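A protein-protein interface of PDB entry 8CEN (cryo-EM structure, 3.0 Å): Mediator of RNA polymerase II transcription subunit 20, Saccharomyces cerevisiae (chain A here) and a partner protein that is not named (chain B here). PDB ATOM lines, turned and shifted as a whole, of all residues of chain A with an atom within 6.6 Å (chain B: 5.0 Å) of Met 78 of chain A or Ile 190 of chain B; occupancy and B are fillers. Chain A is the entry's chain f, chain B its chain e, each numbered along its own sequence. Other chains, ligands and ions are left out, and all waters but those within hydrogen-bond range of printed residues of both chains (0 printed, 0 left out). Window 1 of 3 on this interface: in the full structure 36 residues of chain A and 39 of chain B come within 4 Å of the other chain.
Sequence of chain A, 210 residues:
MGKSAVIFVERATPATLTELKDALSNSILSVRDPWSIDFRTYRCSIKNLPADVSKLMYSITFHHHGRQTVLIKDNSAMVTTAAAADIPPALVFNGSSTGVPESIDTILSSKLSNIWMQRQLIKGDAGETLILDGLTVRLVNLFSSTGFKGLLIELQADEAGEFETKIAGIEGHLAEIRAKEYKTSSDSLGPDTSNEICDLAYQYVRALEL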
ATOM      1  N   MET A  57      11.165  -3.892 -28.618  1.00  0.00           N
ATOM      2  CA  MET A  57      11.791  -2.665 -28.138  1.00  0.00           C
ATOM      3  C   MET A  57      10.873  -1.499 -28.461  1.00  0.00           C
ATOM      4  O   MET A  57      10.489  -1.310 -29.619  1.00  0.00           O
ATOM      5  CB  MET A  57      13.175  -2.466 -28.763  1.00  0.00           C
ATOM      6  CG  MET A  57      13.915  -1.236 -28.270  1.00  0.00           C
ATOM      7  SD  MET A  57      15.546  -1.077 -29.021  1.00  0.00           S
ATOM      8  CE  MET A  57      15.108  -0.614 -30.691  1.00  0.00           C
ATOM      9  N   THR A  69      13.527  10.914 -26.884  1.00  0.00           N
ATOM     10  CA  THR A  69      13.129   9.551 -27.209  1.00  0.00           C
ATOM     11  C   THR A  69      13.692   8.588 -26.175  1.00  0.00           C
ATOM     12  O   THR A  69      14.894   8.604 -25.894  1.00  0.00           O
ATOM     13  CB  THR A  69      13.620   9.159 -28.606  1.00  0.00           C
ATOM     14  OG1 THR A  69      13.165  10.120 -29.566  1.00  0.00           O
ATOM     15  CG2 THR A  69      13.111   7.783 -28.983  1.00  0.00           C
ATOM     16  N   VAL A  70      12.832   7.738 -25.625  1.00  0.00           N
ATOM     17  CA  VAL A  70      13.234   6.724 -24.659  1.00  0.00           C
ATOM     18  C   VAL A  70      13.041   5.353 -25.285  1.00  0.00           C
ATOM     19  O   VAL A  70      11.982   5.065 -25.856  1.00  0.00           O
ATOM     20  CB  VAL A  70      12.442   6.843 -23.346  1.00  0.00           C
ATOM     21  CG1 VAL A  70      13.041   5.936 -22.284  1.00  0.00           C
ATOM     22  CG2 VAL A  70      12.431   8.276 -22.874  1.00  0.00           C
ATOM     23  N   LEU A  71      14.067   4.515 -25.186  1.00  0.00           N
ATOM     24  CA  LEU A  71      14.015   3.137 -25.652  1.00  0.00           C
ATOM     25  C   LEU A  71      13.835   2.214 -24.455  1.00  0.00           C
ATOM     26  O   LEU A  71      14.608   2.280 -23.494  1.00  0.00           O
ATOM     27  CB  LEU A  71      15.283   2.768 -26.425  1.00  0.00           C
ATOM     28  CG  LEU A  71      15.236   2.840 -27.955  1.00  0.00           C
ATOM     29  CD1 LEU A  71      14.817   4.220 -28.439  1.00  0.00           C
ATOM     30  CD2 LEU A  71      16.577   2.448 -28.555  1.00  0.00           C
ATOM     31  N   ILE A  72      12.813   1.366 -24.518  1.00  0.00           N
ATOM     32  CA  ILE A  72      12.455   0.445 -23.446  1.00  0.00           C
ATOM     33  C   ILE A  72      12.610  -0.974 -23.971  1.00  0.00           C
ATOM     34  O   ILE A  72      12.068  -1.311 -25.030  1.00  0.00           O
ATOM     35  CB  ILE A  72      11.017   0.681 -22.947  1.00  0.00           C
ATOM     36  CG1 ILE A  72      10.781   2.162 -22.642  1.00  0.00           C
ATOM     37  CG2 ILE A  72      10.724  -0.185 -21.729  1.00  0.00           C
ATOM     38  CD1 ILE A  72      11.463   2.646 -21.386  1.00  0.00           C
ATOM     39  N   LYS A  73      13.347  -1.799 -23.227  1.00  0.00           N
ATOM     40  CA  LYS A  73      13.548  -3.199 -23.590  1.00  0.00           C
ATOM     41  C   LYS A  73      13.915  -3.979 -22.338  1.00  0.00           C
ATOM     42  O   LYS A  73      14.925  -3.666 -21.697  1.00  0.00           O
ATOM     43  CB  LYS A  73      14.642  -3.343 -24.647  1.00  0.00           C
ATOM     44  CG  LYS A  73      15.041  -4.783 -24.922  1.00  0.00           C
ATOM     45  CD  LYS A  73      16.207  -4.862 -25.892  1.00  0.00           C
ATOM     46  CE  LYS A  73      16.504  -6.302 -26.276  1.00  0.00           C
ATOM     47  NZ  LYS A  73      17.012  -7.092 -25.120  1.00  0.00           N
ATOM     48  N   SER A  76      14.529  -2.199 -19.212  1.00  0.00           N
ATOM     49  CA  SER A  76      15.723  -1.370 -19.297  1.00  0.00           C
ATOM     50  C   SER A  76      15.400  -0.157 -20.153  1.00  0.00           C
ATOM     51  O   SER A  76      14.860  -0.299 -21.255  1.00  0.00           O
ATOM     52  CB  SER A  76      16.903  -2.146 -19.890  1.00  0.00           C
ATOM     53  OG  SER A  76      16.785  -2.257 -21.297  1.00  0.00           O
ATOM     54  N   ALA A  77      15.732   1.028 -19.650  1.00  0.00           N
ATOM     55  CA  ALA A  77      15.390   2.280 -20.305  1.00  0.00           C
ATOM     56  C   ALA A  77      16.649   3.012 -20.743  1.00  0.00           C
ATOM     57  O   ALA A  77      17.693   2.937 -20.089  1.00  0.00           O
ATOM     58  CB  ALA A  77      14.564   3.182 -19.382  1.00  0.00           C
ATOM     59  N   MET A  78      16.538   3.717 -21.866  1.00  0.00           N
ATOM     60  CA  MET A  78      17.622   4.545 -22.381  1.00  0.00           C
ATOM     61  C   MET A  78      17.036   5.859 -22.872  1.00  0.00           C
ATOM     62  O   MET A  78      16.215   5.862 -23.792  1.00  0.00           O
ATOM     63  CB  MET A  78      18.371   3.847 -23.517  1.00  0.00           C
ATOM     64  CG  MET A  78      19.495   4.681 -24.102  1.00  0.00           C
ATOM     65  SD  MET A  78      20.631   3.703 -25.095  1.00  0.00           S
ATOM     66  CE  MET A  78      19.483   2.941 -26.233  1.00  0.00           C
ATOM     67  N   VAL A  79      17.454   6.963 -22.264  1.00  0.00           N
ATOM     68  CA  VAL A  79      16.993   8.292 -22.648  1.00  0.00           C
ATOM     69  C   VAL A  79      17.960   8.870 -23.672  1.00  0.00           C
ATOM     70  O   VAL A  79      19.180   8.852 -23.466  1.00  0.00           O
ATOM     71  CB  VAL A  79      16.874   9.207 -21.418  1.00  0.00           C
ATOM     72  CG1 VAL A  79      16.335  10.571 -21.816  1.00  0.00           C
ATOM     73  CG2 VAL A  79      15.984   8.565 -20.366  1.00  0.00           C
ATOM     74  N   THR A  80      17.420   9.385 -24.775  1.00  0.00           N
ATOM     75  CA  THR A  80      18.210   9.899 -25.881  1.00  0.00           C
ATOM     76  C   THR A  80      17.565  11.192 -26.360  1.00  0.00           C
ATOM     77  O   THR A  80      16.340  11.339 -26.322  1.00  0.00           O
ATOM     78  CB  THR A  80      18.290   8.853 -27.012  1.00  0.00           C
ATOM     79  OG1 THR A  80      18.818   7.628 -26.487  1.00  0.00           O
ATOM     80  CG2 THR A  80      19.192   9.312 -28.148  1.00  0.00           C
ATOM     81  N   THR A  81      18.392  12.143 -26.785  1.00  0.00           N
ATOM     82  CA  THR A  81      17.903  13.410 -27.303  1.00  0.00           C
ATOM     83  C   THR A  81      18.481  13.661 -28.689  1.00  0.00           C
ATOM     84  O   THR A  81      19.508  13.094 -29.073  1.00  0.00           O
ATOM     85  CB  THR A  81      18.250  14.578 -26.369  1.00  0.00           C
ATOM     86  OG1 THR A  81      17.674  15.787 -26.879  1.00  0.00           O
ATOM     87  CG2 THR A  81      19.756  14.749 -26.249  1.00  0.00           C
ATOM     88  N   LEU A  91      30.014  17.321 -23.615  1.00  0.00           N
ATOM     89  CA  LEU A  91      30.160  16.491 -24.807  1.00  0.00           C
ATOM     90  C   LEU A  91      30.447  17.329 -26.047  1.00  0.00           C
ATOM     91  O   LEU A  91      31.156  16.872 -26.951  1.00  0.00           O
ATOM     92  CB  LEU A  91      28.906  15.642 -25.019  1.00  0.00           C
ATOM     93  CG  LEU A  91      28.603  14.578 -23.961  1.00  0.00           C
ATOM     94  CD1 LEU A  91      27.493  13.654 -24.434  1.00  0.00           C
ATOM     95  CD2 LEU A  91      29.850  13.784 -23.605  1.00  0.00           C
ATOM     96  N   ILE A 104      17.487   8.829 -32.689  1.00  0.00           N
ATOM     97  CA  ILE A 104      17.801   7.410 -32.578  1.00  0.00           C
ATOM     98  C   ILE A 104      16.805   6.575 -33.375  1.00  0.00           C
ATOM     99  O   ILE A 104      17.152   5.496 -33.868  1.00  0.00           O
ATOM    100  CB  ILE A 104      17.869   7.004 -31.090  1.00  0.00           C
ATOM    101  CG1 ILE A 104      18.351   5.560 -30.929  1.00  0.00           C
ATOM    102  CG2 ILE A 104      16.530   7.216 -30.399  1.00  0.00           C
ATOM    103  CD1 ILE A 104      19.767   5.330 -31.412  1.00  0.00           C
ATOM    104  N   CYS A 198      11.942   8.420 -18.070  1.00  0.00           N
ATOM    105  CA  CYS A 198      12.024   6.980 -18.304  1.00  0.00           C
ATOM    106  C   CYS A 198      10.924   6.230 -17.559  1.00  0.00           C
ATOM    107  O   CYS A 198      10.386   5.241 -18.076  1.00  0.00           O
ATOM    108  CB  CYS A 198      13.396   6.449 -17.895  1.00  0.00           C
ATOM    109  SG  CYS A 198      13.742   6.590 -16.140  1.00  0.00           S
ATOM    110  N   LEU B  66      30.942   4.758 -28.392  1.00  0.00           N
ATOM    111  CA  LEU B  66      30.355   5.606 -27.362  1.00  0.00           C
ATOM    112  C   LEU B  66      31.466   6.393 -26.691  1.00  0.00           C
ATOM    113  O   LEU B  66      32.418   5.806 -26.170  1.00  0.00           O
ATOM    114  CB  LEU B  66      29.594   4.777 -26.325  1.00  0.00           C
ATOM    115  CG  LEU B  66      28.076   4.658 -26.475  1.00  0.00           C
ATOM    116  CD1 LEU B  66      27.701   4.037 -27.806  1.00  0.00           C
ATOM    117  CD2 LEU B  66      27.501   3.851 -25.329  1.00  0.00           C
ATOM    118  N   SER B 162      25.871   8.052 -16.840  1.00  0.00           N
ATOM    119  CA  SER B 162      26.402   9.318 -17.309  1.00  0.00           C
ATOM    120  C   SER B 162      25.997   9.555 -18.764  1.00  0.00           C
ATOM    121  O   SER B 162      25.645   8.614 -19.477  1.00  0.00           O
ATOM    122  CB  SER B 162      27.922   9.319 -17.170  1.00  0.00           C
ATOM    123  OG  SER B 162      28.467   8.123 -17.694  1.00  0.00           O
ATOM    124  N   PRO B 163      25.993  10.813 -19.215  1.00  0.00           N
ATOM    125  CA  PRO B 163      25.739  11.077 -20.638  1.00  0.00           C
ATOM    126  C   PRO B 163      26.834  10.505 -21.528  1.00  0.00           C
ATOM    127  O   PRO B 163      28.018  10.527 -21.186  1.00  0.00           O
ATOM    128  CB  PRO B 163      25.701  12.607 -20.715  1.00  0.00           C
ATOM    129  CG  PRO B 163      25.335  13.041 -19.345  1.00  0.00           C
ATOM    130  CD  PRO B 163      25.985  12.056 -18.423  1.00  0.00           C
ATOM    131  N   TRP B 164      26.417   9.995 -22.684  1.00  0.00           N
ATOM    132  CA  TRP B 164      27.318   9.455 -23.691  1.00  0.00           C
ATOM    133  C   TRP B 164      26.977  10.061 -25.043  1.00  0.00           C
ATOM    134  O   TRP B 164      25.884  10.588 -25.251  1.00  0.00           O
ATOM    135  CB  TRP B 164      27.227   7.923 -23.795  1.00  0.00           C
ATOM    136  CG  TRP B 164      27.758   7.168 -22.617  1.00  0.00           C
ATOM    137  CD1 TRP B 164      27.071   6.819 -21.494  1.00  0.00           C
ATOM    138  CD2 TRP B 164      29.081   6.642 -22.457  1.00  0.00           C
ATOM    139  NE1 TRP B 164      27.886   6.120 -20.637  1.00  0.00           N
ATOM    140  CE2 TRP B 164      29.125   5.998 -21.207  1.00  0.00           C
ATOM    141  CE3 TRP B 164      30.233   6.660 -23.249  1.00  0.00           C
ATOM    142  CZ2 TRP B 164      30.276   5.375 -20.728  1.00  0.00           C
ATOM    143  CZ3 TRP B 164      31.375   6.042 -22.771  1.00  0.00           C
ATOM    144  CH2 TRP B 164      31.388   5.410 -21.523  1.00  0.00           C
ATOM    145  N   SER B 165      27.922   9.963 -25.973  1.00  0.00           N
ATOM    146  CA  SER B 165      27.703  10.337 -27.363  1.00  0.00           C
ATOM    147  C   SER B 165      27.904   9.095 -28.214  1.00  0.00           C
ATOM    148  O   SER B 165      28.998   8.521 -28.230  1.00  0.00           O
ATOM    149  CB  SER B 165      28.656  11.454 -27.793  1.00  0.00           C
ATOM    150  OG  SER B 165      28.630  11.636 -29.197  1.00  0.00           O
ATOM    151  N   LEU B 166      26.848   8.677 -28.903  1.00  0.00           N
ATOM    152  CA  LEU B 166      26.876   7.500 -29.761  1.00  0.00           C
ATOM    153  C   LEU B 166      27.203   7.945 -31.179  1.00  0.00           C
ATOM    154  O   LEU B 166      26.374   8.586 -31.831  1.00  0.00           O
ATOM    155  CB  LEU B 166      25.531   6.772 -29.720  1.00  0.00           C
ATOM    156  CG  LEU B 166      25.350   5.427 -30.432  1.00  0.00           C
ATOM    157  CD1 LEU B 166      24.472   4.511 -29.602  1.00  0.00           C
ATOM    158  CD2 LEU B 166      24.745   5.607 -31.817  1.00  0.00           C
ATOM    159  N   THR B 188      24.084  10.358 -31.720  1.00  0.00           N
ATOM    160  CA  THR B 188      23.069  10.711 -30.738  1.00  0.00           C
ATOM    161  C   THR B 188      23.730  11.068 -29.416  1.00  0.00           C
ATOM    162  O   THR B 188      24.917  10.815 -29.194  1.00  0.00           O
ATOM    163  CB  THR B 188      22.078   9.564 -30.504  1.00  0.00           C
ATOM    164  OG1 THR B 188      22.775   8.422 -29.998  1.00  0.00           O
ATOM    165  CG2 THR B 188      21.374   9.187 -31.773  1.00  0.00           C
ATOM    166  N   ILE B 189      22.930  11.633 -28.520  1.00  0.00           N
ATOM    167  CA  ILE B 189      23.348  11.907 -27.152  1.00  0.00           C
ATOM    168  C   ILE B 189      22.495  11.043 -26.236  1.00  0.00           C
ATOM    169  O   ILE B 189      21.304  11.317 -26.040  1.00  0.00           O
ATOM    170  CB  ILE B 189      23.216  13.392 -26.793  1.00  0.00           C
ATOM    171  CG1 ILE B 189      23.990  14.251 -27.795  1.00  0.00           C
ATOM    172  CG2 ILE B 189      23.696  13.639 -25.368  1.00  0.00           C
ATOM    173  CD1 ILE B 189      25.492  14.168 -27.646  1.00  0.00           C
ATOM    174  N   ILE B 190      23.101  10.003 -25.674  1.00  0.00           N
ATOM    175  CA  ILE B 190      22.432   9.153 -24.697  1.00  0.00           C
ATOM    176  C   ILE B 190      22.450   9.882 -23.360  1.00  0.00           C
ATOM    177  O   ILE B 190      23.519  10.132 -22.796  1.00  0.00           O
ATOM    178  CB  ILE B 190      23.119   7.786 -24.592  1.00  0.00           C
ATOM    179  CG1 ILE B 190      22.955   7.006 -25.897  1.00  0.00           C
ATOM    180  CG2 ILE B 190      22.556   6.993 -23.423  1.00  0.00           C
ATOM    181  CD1 ILE B 190      23.635   5.658 -25.890  1.00  0.00           C
ATOM    182  N   LEU B 191      21.266  10.227 -22.856  1.00  0.00           N
ATOM    183  CA  LEU B 191      21.168  11.118 -21.706  1.00  0.00           C
ATOM    184  C   LEU B 191      21.169  10.368 -20.378  1.00  0.00           C
ATOM    185  O   LEU B 191      22.003  10.645 -19.511  1.00  0.00           O
ATOM    186  CB  LEU B 191      19.906  11.978 -21.823  1.00  0.00           C
ATOM    187  CG  LEU B 191      20.038  13.247 -22.667  1.00  0.00           C
ATOM    188  CD1 LEU B 191      18.740  14.038 -22.649  1.00  0.00           C
ATOM    189  CD2 LEU B 191      21.197  14.100 -22.178  1.00  0.00           C
ATOM    190  N   SER B 192      20.247   9.427 -20.198  1.00  0.00           N
ATOM    191  CA  SER B 192      20.095   8.764 -18.911  1.00  0.00           C
ATOM    192  C   SER B 192      19.593   7.343 -19.127  1.00  0.00           C
ATOM    193  O   SER B 192      19.222   6.951 -20.236  1.00  0.00           O
ATOM    194  CB  SER B 192      19.147   9.546 -17.996  1.00  0.00           C
ATOM    195  OG  SER B 192      18.986   8.894 -16.749  1.00  0.00           O
ATOM    196  N   SER B 193      19.586   6.572 -18.040  1.00  0.00           N
ATOM    197  CA  SER B 193      19.163   5.180 -18.076  1.00  0.00           C
ATOM    198  C   SER B 193      18.629   4.796 -16.704  1.00  0.00           C
ATOM    199  O   SER B 193      18.925   5.447 -15.700  1.00  0.00           O
ATOM    200  CB  SER B 193      20.315   4.254 -18.480  1.00  0.00           C
ATOM    201  OG  SER B 193      20.789   4.570 -19.777  1.00  0.00           O
ATOM    202  N   LEU B 203      22.795  -2.344 -22.030  1.00  0.00           N
ATOM    203  CA  LEU B 203      21.954  -1.691 -23.032  1.00  0.00           C
ATOM    204  C   LEU B 203      22.506  -1.902 -24.436  1.00  0.00           C
ATOM    205  O   LEU B 203      21.748  -2.157 -25.381  1.00  0.00           O
ATOM    206  CB  LEU B 203      21.832  -0.198 -22.733  1.00  0.00           C
ATOM    207  CG  LEU B 203      21.101   0.208 -21.456  1.00  0.00           C
ATOM    208  CD1 LEU B 203      21.206   1.704 -21.264  1.00  0.00           C
ATOM    209  CD2 LEU B 203      19.647  -0.224 -21.515  1.00  0.00           C
ATOM    210  N   LEU B 207      20.699  -3.747 -27.625  1.00  0.00           N
ATOM    211  CA  LEU B 207      20.716  -3.373 -29.038  1.00  0.00           C
ATOM    212  C   LEU B 207      21.519  -4.341 -29.901  1.00  0.00           C
ATOM    213  O   LEU B 207      21.397  -4.287 -31.129  1.00  0.00           O
ATOM    214  CB  LEU B 207      21.247  -1.948 -29.244  1.00  0.00           C
ATOM    215  CG  LEU B 207      20.347  -0.734 -28.974  1.00  0.00           C
ATOM    216  CD1 LEU B 207      20.059  -0.478 -27.511  1.00  0.00           C
ATOM    217  CD2 LEU B 207      20.953   0.508 -29.620  1.00  0.00           C
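The backbone NH (N) of Ile 190 of chain B lies within hydrogen-bond range of the backbone carbonyl oxygen (O) of Trp 164 of chain B (2.9 Å). N of Leu 166 of chain B lies within hydrogen-bond range of O of Thr 188 of chain B, 2.9 Å away. The backbone carbonyl oxygen of Thr 69 of chain A is in hydrogen-bond range of the backbone NH of Thr 80 of chain A (2.9 Å). The backbone NH of Leu 71 of chain A lies within hydrogen-bond range of the backbone carbonyl oxygen of Met 78 of chain A.
Met 78 of chain A touches three residues of chain B. Of chain A, only Met 78 (3.7 Å) and Val 79 (3.4 Å) come within 4 Å of Ile 190 of chain B. Printed residues of chain B within 4 Å of Leu 91 of chain A: Trp 164 (3.6 Å) and Ile 189 (3.8 Å). Of the printed residues of chain A, Thr 188 of chain B touches Thr 80. The nearest residue of chain A that does not touch Ile 190 of chain B is Thr 80 of chain A (4.2 Å). The nearest printed residue of chain A that does not touch Leu 191 of chain B is Thr 80 of chain A (4.3 Å).
O of Ile 189 of chain B sits at hydrogen-bond distance from N of Thr 81 of chain A. The backbone NH (N) of Leu 191 of chain B sits at hydrogen-bond distance from the backbone carbonyl oxygen (O) of Val 79 of chain A, 2.6 Å away. O of Ser 192 of chain B sits at hydrogen-bond distance from N of Val 79 of chain A (2.7 Å).
OG of Ser 76 of chain A touches CD2 of Leu 203 of chain B, 3.5 Å away. CB of Ser 193 of chain B touches O of Ala 77 of chain A (3.3 Å). Ala 77 of chain A touches Leu 203 of chain B. Met 78 of chain A touches Ile 190 of chain B. Ser 192 of chain B touches Met 78 of chain A (O to C, 3.6 Å). Leu 207 of chain B touches Met 78 of chain A (CD1 to CE, 3.7 Å). Val 79 of chain A touches Ile 190 of chain B. Thr 80 of chain A touches Ile 189 of chain B. Leu 191 of chain B touches Thr 81 of chain A. Leu 91 of chain A touches Trp 164 of chain B (CD1 to O, 3.6 Å).
Printed residues of chain B that touch a printed residue of chain A: Trp 164, Thr 188, Ile 189, Ile 190, Leu 191, Ser 192, Ser 193, Leu 203 and Leu 207. Hydrophobic or aromatic side chains of chain B within 4 Å of the printed part of chain A: Ile 189, Ile 190, Leu 191, Leu 203 and Leu 207. Of the 15 printed residues of chain A, 7 touch a printed residue of chain B. Among the printed residues, 15 pairs touch across the chains.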
